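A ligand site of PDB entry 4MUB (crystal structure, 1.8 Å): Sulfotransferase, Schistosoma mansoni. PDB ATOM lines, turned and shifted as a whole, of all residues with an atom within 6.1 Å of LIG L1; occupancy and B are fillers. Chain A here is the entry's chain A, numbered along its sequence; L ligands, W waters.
The side-chain carboxylate (OD2) of Asp 93 sits at hydrogen-bond distance from an oxygen (O3) of LG2 L2, 2.5 Å away.
An oxygen (O6) of LIG L1 lies within salt-bridge range of the guanidinium group of Arg 19 (2.9 Å).
The backbone NH (N) of Lys 23 sits at hydrogen-bond distance from an oxygen (O4) of LIG L1 (2.9 Å).
N of Arg 19 lies within hydrogen-bond range of O5 of LIG L1, at 3.0 Å.
The backbone NH of Thr 20 lies within hydrogen-bond range of an oxygen (O5) of LIG L1.
The backbone NH (N) of Thr 22 is in hydrogen-bond range of an oxygen (O5) of LIG L1 (2.7 Å).
The side-chain hydroxyl (OG) of Ser 24 lies within hydrogen-bond range of a nitrogen (N2) of LIG L1 (2.8 Å).
The backbone carbonyl oxygen of Pro 227 lies within hydrogen-bond range of a nitrogen (N3) of LIG L1, 3.0 Å away.
The guanidinium group (NH2) of Arg 117 lies within salt-bridge range of an oxygen (O2) of LIG L1 (2.8 Å).
O1 of LIG L1 lies within hydrogen-bond range of OG of Ser 125 (2.5 Å).
The backbone NH of His 232 lies within hydrogen-bond range of an oxygen (O1) of LIG L1 (2.9 Å).
O7 of LIG L1 lies within hydrogen-bond range of N of Gly 21 (2.9 Å).
ND2 of Asn 230 lies within hydrogen-bond range of O4 of LIG L1 (2.9 Å).
The side-chain hydroxyl (OG1) of Thr 22 is in hydrogen-bond range of an oxygen (O5) of LIG L1, at 2.6 Å.
The guanidinium group (NE) of Arg 19 sits at hydrogen-bond distance from the side-chain hydroxyl (OG) of Ser 125 (2.7 Å).
OG of Ser 24 is in hydrogen-bond range of N of Val 229 (3.0 Å).
NE2 of His 39 is in hydrogen-bond range of OG1 of Thr 22 (2.9 Å).
The guanidinium group (NH2) of Arg 19 is in hydrogen-bond range of the backbone carbonyl oxygen (O) of Asn 230, 2.8 Å away.
OG of Ser 24 sits at hydrogen-bond distance from O of Pro 227, 3.1 Å away.
The guanidinium group of Arg 117 sits at hydrogen-bond distance from the backbone carbonyl oxygen of Arg 19 (2.9 Å).
The backbone NH (N) of Lys 23 is in hydrogen-bond range of a ring nitrogen (NE2) of His 39 (3.4 Å).
OG1 of Thr 20 lies within hydrogen-bond range of O of Leu 17 (2.6 Å).
Residues that only touch LIG L1: Val 229 (3.4 Å), Leu 205 (3.4 Å), Ser 231 (3.5 Å), Cys 228 (3.7 Å), Tyr 226 (3.8 Å), Pro 18 (3.9 Å) and Gly 206 (3.9 Å).
Hydrophobic or aromatic side chains that line LIG L1: Leu 205, Tyr 226 and His 232.
Of the 26 residues printed, 18 come within 4 Å of LIG L1.
Water W1 bridges O2 of LIG L1 (2.6 Å) and O of Asp 121 (2.8 Å).
Water W8 lies within hydrogen-bond range of O3 of LG2 L2, O6 of LIG L1, ND2 of Asn 230 and NH1 of Arg 19.
Water W6 lies within hydrogen-bond range of an oxygen (O4) of LIG L1 (2.8 Å), the backbone NH (N) of Ser 24 (2.9 Å), the backbone carbonyl oxygen (O) of Val 229 (2.9 Å) and the backbone NH (N) of Lys 23 (3.4 Å).
Water W9 lies within hydrogen-bond range of O10 of LIG L1 (3.0 Å) and SG of Cys 228 (3.6 Å).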
ATOM      1  N   LEU A  17      -5.092 -12.181 -22.450  1.00  0.00           N
ATOM      2  CA  LEU A  17      -5.547 -11.033 -21.670  1.00  0.00           C
ATOM      3  C   LEU A  17      -6.770 -11.405 -20.838  1.00  0.00           C
ATOM      4  O   LEU A  17      -7.436 -12.408 -21.093  1.00  0.00           O
ATOM      5  CB  LEU A  17      -5.898  -9.884 -22.623  1.00  0.00           C
ATOM      6  CG  LEU A  17      -4.681  -9.326 -23.361  1.00  0.00           C
ATOM      7  CD1 LEU A  17      -5.161  -8.446 -24.521  1.00  0.00           C
ATOM      8  CD2 LEU A  17      -3.826  -8.554 -22.382  1.00  0.00           C
ATOM      9  N   PRO A  18      -7.061 -10.612 -19.812  1.00  0.00           N
ATOM     10  CA  PRO A  18      -8.274 -10.882 -19.045  1.00  0.00           C
ATOM     11  C   PRO A  18      -9.520 -10.883 -19.924  1.00  0.00           C
ATOM     12  O   PRO A  18      -9.560 -10.188 -20.957  1.00  0.00           O
ATOM     13  CB  PRO A  18      -8.340  -9.704 -18.059  1.00  0.00           C
ATOM     14  CG  PRO A  18      -7.268  -8.737 -18.483  1.00  0.00           C
ATOM     15  CD  PRO A  18      -6.243  -9.544 -19.198  1.00  0.00           C
ATOM     16  N   ARG A  19     -10.509 -11.650 -19.501  1.00  0.00           N
ATOM     17  CA  ARG A  19     -11.792 -11.821 -20.203  1.00  0.00           C
ATOM     18  C   ARG A  19     -11.659 -12.632 -21.483  1.00  0.00           C
ATOM     19  O   ARG A  19     -12.455 -12.466 -22.403  1.00  0.00           O
ATOM     20  CB  ARG A  19     -12.513 -10.489 -20.477  1.00  0.00           C
ATOM     21  CG  ARG A  19     -12.621  -9.541 -19.282  1.00  0.00           C
ATOM     22  CD  ARG A  19     -13.106 -10.268 -18.024  1.00  0.00           C
ATOM     23  NE  ARG A  19     -14.484 -10.755 -18.182  1.00  0.00           N
ATOM     24  CZ  ARG A  19     -15.102 -11.535 -17.305  1.00  0.00           C
ATOM     25  NH1 ARG A  19     -14.451 -11.946 -16.215  1.00  0.00           N
ATOM     26  NH2 ARG A  19     -16.353 -11.928 -17.514  1.00  0.00           N
ATOM     27  N   THR A  20     -10.696 -13.547 -21.520  1.00  0.00           N
ATOM     28  CA  THR A  20     -10.524 -14.453 -22.648  1.00  0.00           C
ATOM     29  C   THR A  20     -10.588 -15.912 -22.226  1.00  0.00           C
ATOM     30  O   THR A  20     -10.100 -16.793 -22.939  1.00  0.00           O
ATOM     31  CB  THR A  20      -9.197 -14.201 -23.437  1.00  0.00           C
ATOM     32  OG1 THR A  20      -8.068 -14.464 -22.586  1.00  0.00           O
ATOM     33  CG2 THR A  20      -9.130 -12.757 -23.925  1.00  0.00           C
ATOM     34  N   GLY A  21     -11.209 -16.173 -21.079  1.00  0.00           N
ATOM     35  CA  GLY A  21     -11.318 -17.543 -20.594  1.00  0.00           C
ATOM     36  C   GLY A  21     -10.183 -17.950 -19.677  1.00  0.00           C
ATOM     37  O   GLY A  21      -9.891 -19.145 -19.534  1.00  0.00           O
ATOM     38  N   THR A  22      -9.551 -16.963 -19.032  1.00  0.00           N
ATOM     39  CA  THR A  22      -8.397 -17.248 -18.157  1.00  0.00           C
ATOM     40  C   THR A  22      -8.745 -18.019 -16.890  1.00  0.00           C
ATOM     41  O   THR A  22      -7.950 -18.837 -16.421  1.00  0.00           O
ATOM     42  CB  THR A  22      -7.626 -15.975 -17.750  1.00  0.00           C
ATOM     43  OG1 THR A  22      -8.480 -15.109 -16.980  1.00  0.00           O
ATOM     44  CG2 THR A  22      -7.119 -15.248 -18.968  1.00  0.00           C
ATOM     45  N   LYS A  23      -9.909 -17.751 -16.315  1.00  0.00           N
ATOM     46  CA  LYS A  23     -10.296 -18.452 -15.081  1.00  0.00           C
ATOM     47  C   LYS A  23     -10.683 -19.909 -15.377  1.00  0.00           C
ATOM     48  O   LYS A  23     -10.334 -20.807 -14.611  1.00  0.00           O
ATOM     49  CB  LYS A  23     -11.428 -17.709 -14.351  1.00  0.00           C
ATOM     50  CG  LYS A  23     -11.849 -18.348 -13.015  1.00  0.00           C
ATOM     51  CD  LYS A  23     -10.616 -18.561 -12.136  1.00  0.00           C
ATOM     52  CE  LYS A  23     -10.955 -18.712 -10.650  1.00  0.00           C
ATOM     53  NZ  LYS A  23     -11.632 -19.982 -10.290  1.00  0.00           N
ATOM     54  N   SER A  24     -11.382 -20.143 -16.476  1.00  0.00           N
ATOM     55  CA  SER A  24     -11.671 -21.511 -16.884  1.00  0.00           C
ATOM     56  C   SER A  24     -10.375 -22.262 -17.141  1.00  0.00           C
ATOM     57  O   SER A  24     -10.242 -23.424 -16.777  1.00  0.00           O
ATOM     58  CB  SER A  24     -12.571 -21.562 -18.123  1.00  0.00           C
ATOM     59  OG  SER A  24     -13.885 -21.152 -17.790  1.00  0.00           O
ATOM     60  N   HIS A  39      -3.467 -16.477 -11.174  1.00  0.00           N
ATOM     61  CA  HIS A  39      -4.559 -15.771 -11.837  1.00  0.00           C
ATOM     62  C   HIS A  39      -4.784 -14.532 -10.985  1.00  0.00           C
ATOM     63  O   HIS A  39      -4.314 -14.501  -9.853  1.00  0.00           O
ATOM     64  CB  HIS A  39      -5.822 -16.627 -11.803  1.00  0.00           C
ATOM     65  CG  HIS A  39      -6.954 -16.087 -12.611  1.00  0.00           C
ATOM     66  ND1 HIS A  39      -7.898 -15.224 -12.087  1.00  0.00           N
ATOM     67  CD2 HIS A  39      -7.318 -16.282 -13.904  1.00  0.00           C
ATOM     68  CE1 HIS A  39      -8.784 -14.913 -13.020  1.00  0.00           C
ATOM     69  NE2 HIS A  39      -8.446 -15.541 -14.139  1.00  0.00           N
ATOM     70  N   ASP A  93      -3.590 -14.630 -16.822  1.00  0.00           N
ATOM     71  CA  ASP A  93      -4.255 -13.375 -16.443  1.00  0.00           C
ATOM     72  C   ASP A  93      -3.281 -12.243 -16.086  1.00  0.00           C
ATOM     73  O   ASP A  93      -2.070 -12.458 -15.948  1.00  0.00           O
ATOM     74  CB  ASP A  93      -5.198 -13.654 -15.274  1.00  0.00           C
ATOM     75  CG  ASP A  93      -6.254 -12.598 -15.100  1.00  0.00           C
ATOM     76  OD1 ASP A  93      -6.380 -11.701 -15.972  1.00  0.00           O
ATOM     77  OD2 ASP A  93      -6.991 -12.685 -14.097  1.00  0.00           O
ATOM     78  N   ARG A 117     -10.412 -14.274 -28.376  1.00  0.00           N
ATOM     79  CA  ARG A 117     -11.833 -14.286 -28.699  1.00  0.00           C
ATOM     80  C   ARG A 117     -12.147 -13.072 -29.552  1.00  0.00           C
ATOM     81  O   ARG A 117     -11.288 -12.205 -29.780  1.00  0.00           O
ATOM     82  CB  ARG A 117     -12.682 -14.286 -27.419  1.00  0.00           C
ATOM     83  CG  ARG A 117     -12.685 -12.928 -26.726  1.00  0.00           C
ATOM     84  CD  ARG A 117     -13.383 -12.984 -25.382  1.00  0.00           C
ATOM     85  NE  ARG A 117     -14.813 -13.254 -25.475  1.00  0.00           N
ATOM     86  CZ  ARG A 117     -15.651 -13.111 -24.448  1.00  0.00           C
ATOM     87  NH1 ARG A 117     -15.177 -12.686 -23.286  1.00  0.00           N
ATOM     88  NH2 ARG A 117     -16.945 -13.371 -24.585  1.00  0.00           N
ATOM     89  N   ASP A 121     -16.671  -8.777 -28.287  1.00  0.00           N
ATOM     90  CA  ASP A 121     -17.116  -9.570 -27.145  1.00  0.00           C
ATOM     91  C   ASP A 121     -16.165  -9.357 -25.971  1.00  0.00           C
ATOM     92  O   ASP A 121     -16.601  -9.272 -24.819  1.00  0.00           O
ATOM     93  CB  ASP A 121     -17.124 -11.060 -27.490  1.00  0.00           C
ATOM     94  CG  ASP A 121     -18.306 -11.466 -28.344  1.00  0.00           C
ATOM     95  OD1 ASP A 121     -19.230 -10.658 -28.527  1.00  0.00           O
ATOM     96  OD2 ASP A 121     -18.290 -12.624 -28.837  1.00  0.00           O
ATOM     97  N   HIS A 124     -16.764  -5.823 -24.487  1.00  0.00           N
ATOM     98  CA  HIS A 124     -18.021  -5.818 -23.743  1.00  0.00           C
ATOM     99  C   HIS A 124     -17.812  -6.455 -22.374  1.00  0.00           C
ATOM    100  O   HIS A 124     -18.218  -5.929 -21.349  1.00  0.00           O
ATOM    101  CB  HIS A 124     -19.101  -6.566 -24.529  1.00  0.00           C
ATOM    102  CG  HIS A 124     -20.428  -6.661 -23.834  1.00  0.00           C
ATOM    103  ND1 HIS A 124     -21.268  -5.580 -23.705  1.00  0.00           N
ATOM    104  CD2 HIS A 124     -21.060  -7.710 -23.269  1.00  0.00           C
ATOM    105  CE1 HIS A 124     -22.366  -5.953 -23.060  1.00  0.00           C
ATOM    106  NE2 HIS A 124     -22.271  -7.244 -22.794  1.00  0.00           N
ATOM    107  N   SER A 125     -17.136  -7.596 -22.374  1.00  0.00           N
ATOM    108  CA  SER A 125     -16.877  -8.316 -21.132  1.00  0.00           C
ATOM    109  C   SER A 125     -15.960  -7.496 -20.192  1.00  0.00           C
ATOM    110  O   SER A 125     -16.212  -7.383 -18.989  1.00  0.00           O
ATOM    111  CB  SER A 125     -16.240  -9.658 -21.471  1.00  0.00           C
ATOM    112  OG  SER A 125     -16.158 -10.481 -20.324  1.00  0.00           O
ATOM    113  N   VAL A 129     -16.744  -5.878 -16.150  1.00  0.00           N
ATOM    114  CA  VAL A 129     -16.082  -6.542 -15.038  1.00  0.00           C
ATOM    115  C   VAL A 129     -14.811  -5.848 -14.558  1.00  0.00           C
ATOM    116  O   VAL A 129     -14.628  -5.591 -13.367  1.00  0.00           O
ATOM    117  CB  VAL A 129     -15.735  -8.007 -15.409  1.00  0.00           C
ATOM    118  CG1 VAL A 129     -14.926  -8.670 -14.301  1.00  0.00           C
ATOM    119  CG2 VAL A 129     -17.015  -8.792 -15.717  1.00  0.00           C
ATOM    120  N   VAL A 130     -13.918  -5.567 -15.500  1.00  0.00           N
ATOM    121  CA  VAL A 130     -12.570  -5.133 -15.178  1.00  0.00           C
ATOM    122  C   VAL A 130     -12.376  -3.621 -15.304  1.00  0.00           C
ATOM    123  O   VAL A 130     -11.700  -2.988 -14.479  1.00  0.00           O
ATOM    124  CB  VAL A 130     -11.565  -5.844 -16.090  1.00  0.00           C
ATOM    125  CG1 VAL A 130     -10.150  -5.330 -15.863  1.00  0.00           C
ATOM    126  CG2 VAL A 130     -11.639  -7.346 -15.878  1.00  0.00           C
ATOM    127  N   LEU A 205     -11.861 -19.206 -27.303  1.00  0.00           N
ATOM    128  CA  LEU A 205     -12.898 -19.520 -26.324  1.00  0.00           C
ATOM    129  C   LEU A 205     -13.788 -20.608 -26.867  1.00  0.00           C
ATOM    130  O   LEU A 205     -14.258 -20.517 -27.996  1.00  0.00           O
ATOM    131  CB  LEU A 205     -13.761 -18.283 -26.052  1.00  0.00           C
ATOM    132  CG  LEU A 205     -13.484 -17.438 -24.834  1.00  0.00           C
ATOM    133  CD1 LEU A 205     -14.631 -16.453 -24.669  1.00  0.00           C
ATOM    134  CD2 LEU A 205     -13.338 -18.315 -23.598  1.00  0.00           C
ATOM    135  N   GLY A 206     -14.021 -21.652 -26.071  1.00  0.00           N
ATOM    136  CA  GLY A 206     -14.864 -22.759 -26.492  1.00  0.00           C
ATOM    137  C   GLY A 206     -14.115 -23.979 -27.021  1.00  0.00           C
ATOM    138  O   GLY A 206     -14.734 -25.032 -27.222  1.00  0.00           O
ATOM    139  N   TYR A 226     -14.957 -29.385 -19.600  1.00  0.00           N
ATOM    140  CA  TYR A 226     -14.027 -28.270 -19.546  1.00  0.00           C
ATOM    141  C   TYR A 226     -14.726 -27.127 -18.815  1.00  0.00           C
ATOM    142  O   TYR A 226     -15.906 -26.868 -19.067  1.00  0.00           O
ATOM    143  CB  TYR A 226     -13.592 -27.843 -20.950  1.00  0.00           C
ATOM    144  CG  TYR A 226     -12.533 -26.787 -20.930  1.00  0.00           C
ATOM    145  CD1 TYR A 226     -11.187 -27.140 -20.862  1.00  0.00           C
ATOM    146  CD2 TYR A 226     -12.861 -25.434 -20.935  1.00  0.00           C
ATOM    147  CE1 TYR A 226     -10.201 -26.170 -20.826  1.00  0.00           C
ATOM    148  CE2 TYR A 226     -11.886 -24.463 -20.890  1.00  0.00           C
ATOM    149  CZ  TYR A 226     -10.562 -24.835 -20.849  1.00  0.00           C
ATOM    150  OH  TYR A 226      -9.585 -23.866 -20.791  1.00  0.00           O
ATOM    151  N   PRO A 227     -14.017 -26.445 -17.904  1.00  0.00           N
ATOM    152  CA  PRO A 227     -14.652 -25.403 -17.081  1.00  0.00           C
ATOM    153  C   PRO A 227     -15.259 -24.279 -17.913  1.00  0.00           C
ATOM    154  O   PRO A 227     -14.733 -23.903 -18.961  1.00  0.00           O
ATOM    155  CB  PRO A 227     -13.499 -24.858 -16.241  1.00  0.00           C
ATOM    156  CG  PRO A 227     -12.519 -25.992 -16.169  1.00  0.00           C
ATOM    157  CD  PRO A 227     -12.629 -26.721 -17.470  1.00  0.00           C
ATOM    158  N   CYS A 228     -16.371 -23.750 -17.431  1.00  0.00           N
ATOM    159  CA  CYS A 228     -17.023 -22.639 -18.087  1.00  0.00           C
ATOM    160  C   CYS A 228     -17.505 -21.677 -17.011  1.00  0.00           C
ATOM    161  O   CYS A 228     -18.680 -21.679 -16.649  1.00  0.00           O
ATOM    162  CB  CYS A 228     -18.192 -23.140 -18.929  1.00  0.00           C
ATOM    163  SG  CYS A 228     -18.936 -21.853 -19.896  1.00  0.00           S
ATOM    164  N   VAL A 229     -16.585 -20.870 -16.487  1.00  0.00           N
ATOM    165  CA  VAL A 229     -16.874 -20.011 -15.335  1.00  0.00           C
ATOM    166  C   VAL A 229     -16.470 -18.575 -15.635  1.00  0.00           C
ATOM    167  O   VAL A 229     -15.766 -18.317 -16.614  1.00  0.00           O
ATOM    168  CB  VAL A 229     -16.117 -20.463 -14.068  1.00  0.00           C
ATOM    169  CG1 VAL A 229     -16.580 -21.843 -13.628  1.00  0.00           C
ATOM    170  CG2 VAL A 229     -14.608 -20.459 -14.306  1.00  0.00           C
ATOM    171  N   ASN A 230     -16.909 -17.657 -14.767  1.00  0.00           N
ATOM    172  CA  ASN A 230     -16.469 -16.254 -14.796  1.00  0.00           C
ATOM    173  C   ASN A 230     -17.066 -15.421 -15.931  1.00  0.00           C
ATOM    174  O   ASN A 230     -16.430 -14.487 -16.434  1.00  0.00           O
ATOM    175  CB  ASN A 230     -14.926 -16.171 -14.796  1.00  0.00           C
ATOM    176  CG  ASN A 230     -14.405 -14.870 -14.207  1.00  0.00           C
ATOM    177  OD1 ASN A 230     -15.117 -14.187 -13.468  1.00  0.00           O
ATOM    178  ND2 ASN A 230     -13.163 -14.522 -14.543  1.00  0.00           N
ATOM    179  N   SER A 231     -18.313 -15.729 -16.305  1.00  0.00           N
ATOM    180  CA  SER A 231     -19.039 -14.910 -17.268  1.00  0.00           C
ATOM    181  C   SER A 231     -19.317 -13.564 -16.622  1.00  0.00           C
ATOM    182  O   SER A 231     -19.356 -13.459 -15.395  1.00  0.00           O
ATOM    183  CB  SER A 231     -20.359 -15.576 -17.641  1.00  0.00           C
ATOM    184  OG  SER A 231     -21.246 -15.549 -16.539  1.00  0.00           O
ATOM    185  N   HIS A 232     -19.501 -12.520 -17.418  1.00  0.00           N
ATOM    186  CA  HIS A 232     -19.789 -11.223 -16.803  1.00  0.00           C
ATOM    187  C   HIS A 232     -21.101 -11.263 -15.999  1.00  0.00           C
ATOM    188  O   HIS A 232     -21.236 -10.561 -15.006  1.00  0.00           O
ATOM    189  CB  HIS A 232     -19.782 -10.080 -17.836  1.00  0.00           C
ATOM    190  CG  HIS A 232     -20.898 -10.124 -18.820  1.00  0.00           C
ATOM    191  ND1 HIS A 232     -22.158  -9.611 -18.543  1.00  0.00           N
ATOM    192  CD2 HIS A 232     -20.960 -10.593 -20.092  1.00  0.00           C
ATOM    193  CE1 HIS A 232     -22.933  -9.759 -19.597  1.00  0.00           C
ATOM    194  NE2 HIS A 232     -22.227 -10.358 -20.550  1.00  0.00           N
ATOM    195  N   HIS A 233     -22.030 -12.115 -16.426  1.00  0.00           N
ATOM    196  CA  HIS A 233     -23.295 -12.264 -15.714  1.00  0.00           C
ATOM    197  C   HIS A 233     -23.036 -12.821 -14.310  1.00  0.00           C
ATOM    198  O   HIS A 233     -23.651 -12.367 -13.344  1.00  0.00           O
ATOM    199  CB  HIS A 233     -24.248 -13.198 -16.459  1.00  0.00           C
ATOM    200  CG  HIS A 233     -24.742 -12.667 -17.772  1.00  0.00           C
ATOM    201  ND1 HIS A 233     -25.538 -11.546 -17.882  1.00  0.00           N
ATOM    202  CD2 HIS A 233     -24.582 -13.144 -19.043  1.00  0.00           C
ATOM    203  CE1 HIS A 233     -25.830 -11.344 -19.159  1.00  0.00           C
ATOM    204  NE2 HIS A 233     -25.272 -12.296 -19.880  1.00  0.00           N
HETATM  205  P1  LIG L   1     -18.220 -13.170 -21.002  1.00  0.00           P
HETATM  206  O1  LIG L   1     -18.030 -12.139 -19.901  1.00  0.00           O
HETATM  207  O2  LIG L   1     -18.456 -12.537 -22.360  1.00  0.00           O
HETATM  208  O3  LIG L   1     -19.387 -14.092 -20.648  1.00  0.00           O
HETATM  209  P2  LIG L   1     -11.766 -14.542 -17.898  1.00  0.00           P
HETATM  210  O4  LIG L   1     -11.850 -15.656 -16.911  1.00  0.00           O
HETATM  211  O5  LIG L   1     -10.400 -14.471 -18.564  1.00  0.00           O
HETATM  212  O6  LIG L   1     -12.099 -13.222 -17.204  1.00  0.00           O
HETATM  213  O7  LIG L   1     -12.791 -14.803 -19.096  1.00  0.00           O
HETATM  214  C1  LIG L   1     -14.202 -14.855 -18.830  1.00  0.00           C
HETATM  215  C2  LIG L   1     -14.908 -14.882 -20.155  1.00  0.00           C
HETATM  216  O8  LIG L   1     -14.674 -16.170 -20.805  1.00  0.00           O
HETATM  217  C3  LIG L   1     -16.393 -14.796 -19.998  1.00  0.00           C
HETATM  218  O9  LIG L   1     -16.924 -14.115 -21.138  1.00  0.00           O
HETATM  219  C4  LIG L   1     -16.794 -16.232 -19.963  1.00  0.00           C
HETATM  220  O10 LIG L   1     -18.169 -16.388 -20.296  1.00  0.00           O
HETATM  221  C5  LIG L   1     -15.931 -16.812 -21.026  1.00  0.00           C
HETATM  222  N1  LIG L   1     -15.707 -18.202 -20.898  1.00  0.00           N
HETATM  223  C6  LIG L   1     -15.031 -18.807 -19.912  1.00  0.00           C
HETATM  224  N2  LIG L   1     -15.014 -20.128 -20.132  1.00  0.00           N
HETATM  225  C7  LIG L   1     -15.686 -20.379 -21.300  1.00  0.00           C
HETATM  226  C8  LIG L   1     -15.994 -21.560 -22.041  1.00  0.00           C
HETATM  227  N3  LIG L   1     -15.578 -22.846 -21.599  1.00  0.00           N
HETATM  228  N4  LIG L   1     -16.697 -21.425 -23.175  1.00  0.00           N
HETATM  229  C9  LIG L   1     -17.102 -20.233 -23.618  1.00  0.00           C
HETATM  230  N5  LIG L   1     -16.843 -19.105 -22.961  1.00  0.00           N
HETATM  231  C10 LIG L   1     -16.139 -19.137 -21.798  1.00  0.00           C
HETATM  232  C1  LG2 L   2     -10.548  -9.905 -12.687  1.00  0.00           C
HETATM  233  C2  LG2 L   2      -9.449  -9.249 -13.297  1.00  0.00           C
HETATM  234  C3  LG2 L   2      -9.135  -7.868 -12.962  1.00  0.00           C
HETATM  235  C4  LG2 L   2      -9.944  -7.177 -11.989  1.00  0.00           C
HETATM  236  C5  LG2 L   2     -11.097  -7.869 -11.355  1.00  0.00           C
HETATM  237  C6  LG2 L   2     -11.378  -9.195 -11.696  1.00  0.00           C
HETATM  238  C7  LG2 L   2     -13.199  -7.745 -10.000  1.00  0.00           C
HETATM  239  C8  LG2 L   2     -13.597  -9.085 -10.471  1.00  0.00           C
HETATM  240  C9  LG2 L   2     -12.568  -9.959 -11.071  1.00  0.00           C
HETATM  241  C10 LG2 L   2      -8.642 -10.043 -14.299  1.00  0.00           C
HETATM  242  C11 LG2 L   2     -13.561  -7.556  -8.527  1.00  0.00           C
HETATM  243  C12 LG2 L   2     -16.457  -8.553  -8.265  1.00  0.00           C
HETATM  244  C13 LG2 L   2     -16.838  -6.335  -7.252  1.00  0.00           C
HETATM  245  C14 LG2 L   2     -15.797  -7.401  -7.597  1.00  0.00           C
HETATM  246  N1  LG2 L   2     -11.936  -7.170 -10.363  1.00  0.00           N
HETATM  247  N2  LG2 L   2      -8.016  -7.192 -13.557  1.00  0.00           N
HETATM  248  N3  LG2 L   2     -14.805  -6.820  -8.492  1.00  0.00           N
HETATM  249  O1  LG2 L   2      -7.177  -6.561 -12.787  1.00  0.00           O
HETATM  250  O2  LG2 L   2      -7.798  -7.202 -14.849  1.00  0.00           O
HETATM  251  O3  LG2 L   2      -9.046 -11.342 -14.209  1.00  0.00           O
HETATM  252  O   HOH W   1     -18.989 -10.452 -23.875  1.00  0.00           O
HETATM  253  O   HOH W   2     -22.031 -14.217 -20.712  1.00  0.00           O
HETATM  254  O   HOH W   3     -18.084 -23.404 -24.463  1.00  0.00           O
HETATM  255  O   HOH W   4     -15.431 -25.345 -23.527  1.00  0.00           O
HETATM  256  O   HOH W   5     -19.978 -14.869 -23.631  1.00  0.00           O
HETATM  257  O   HOH W   6     -13.042 -18.057 -17.685  1.00  0.00           O
HETATM  258  O   HOH W   7     -18.439 -17.177 -24.447  1.00  0.00           O
HETATM  259  O   HOH W   8     -11.462 -12.118 -14.866  1.00  0.00           O
HETATM  260  O   HOH W   9     -20.193 -18.541 -20.150  1.00  0.00           O
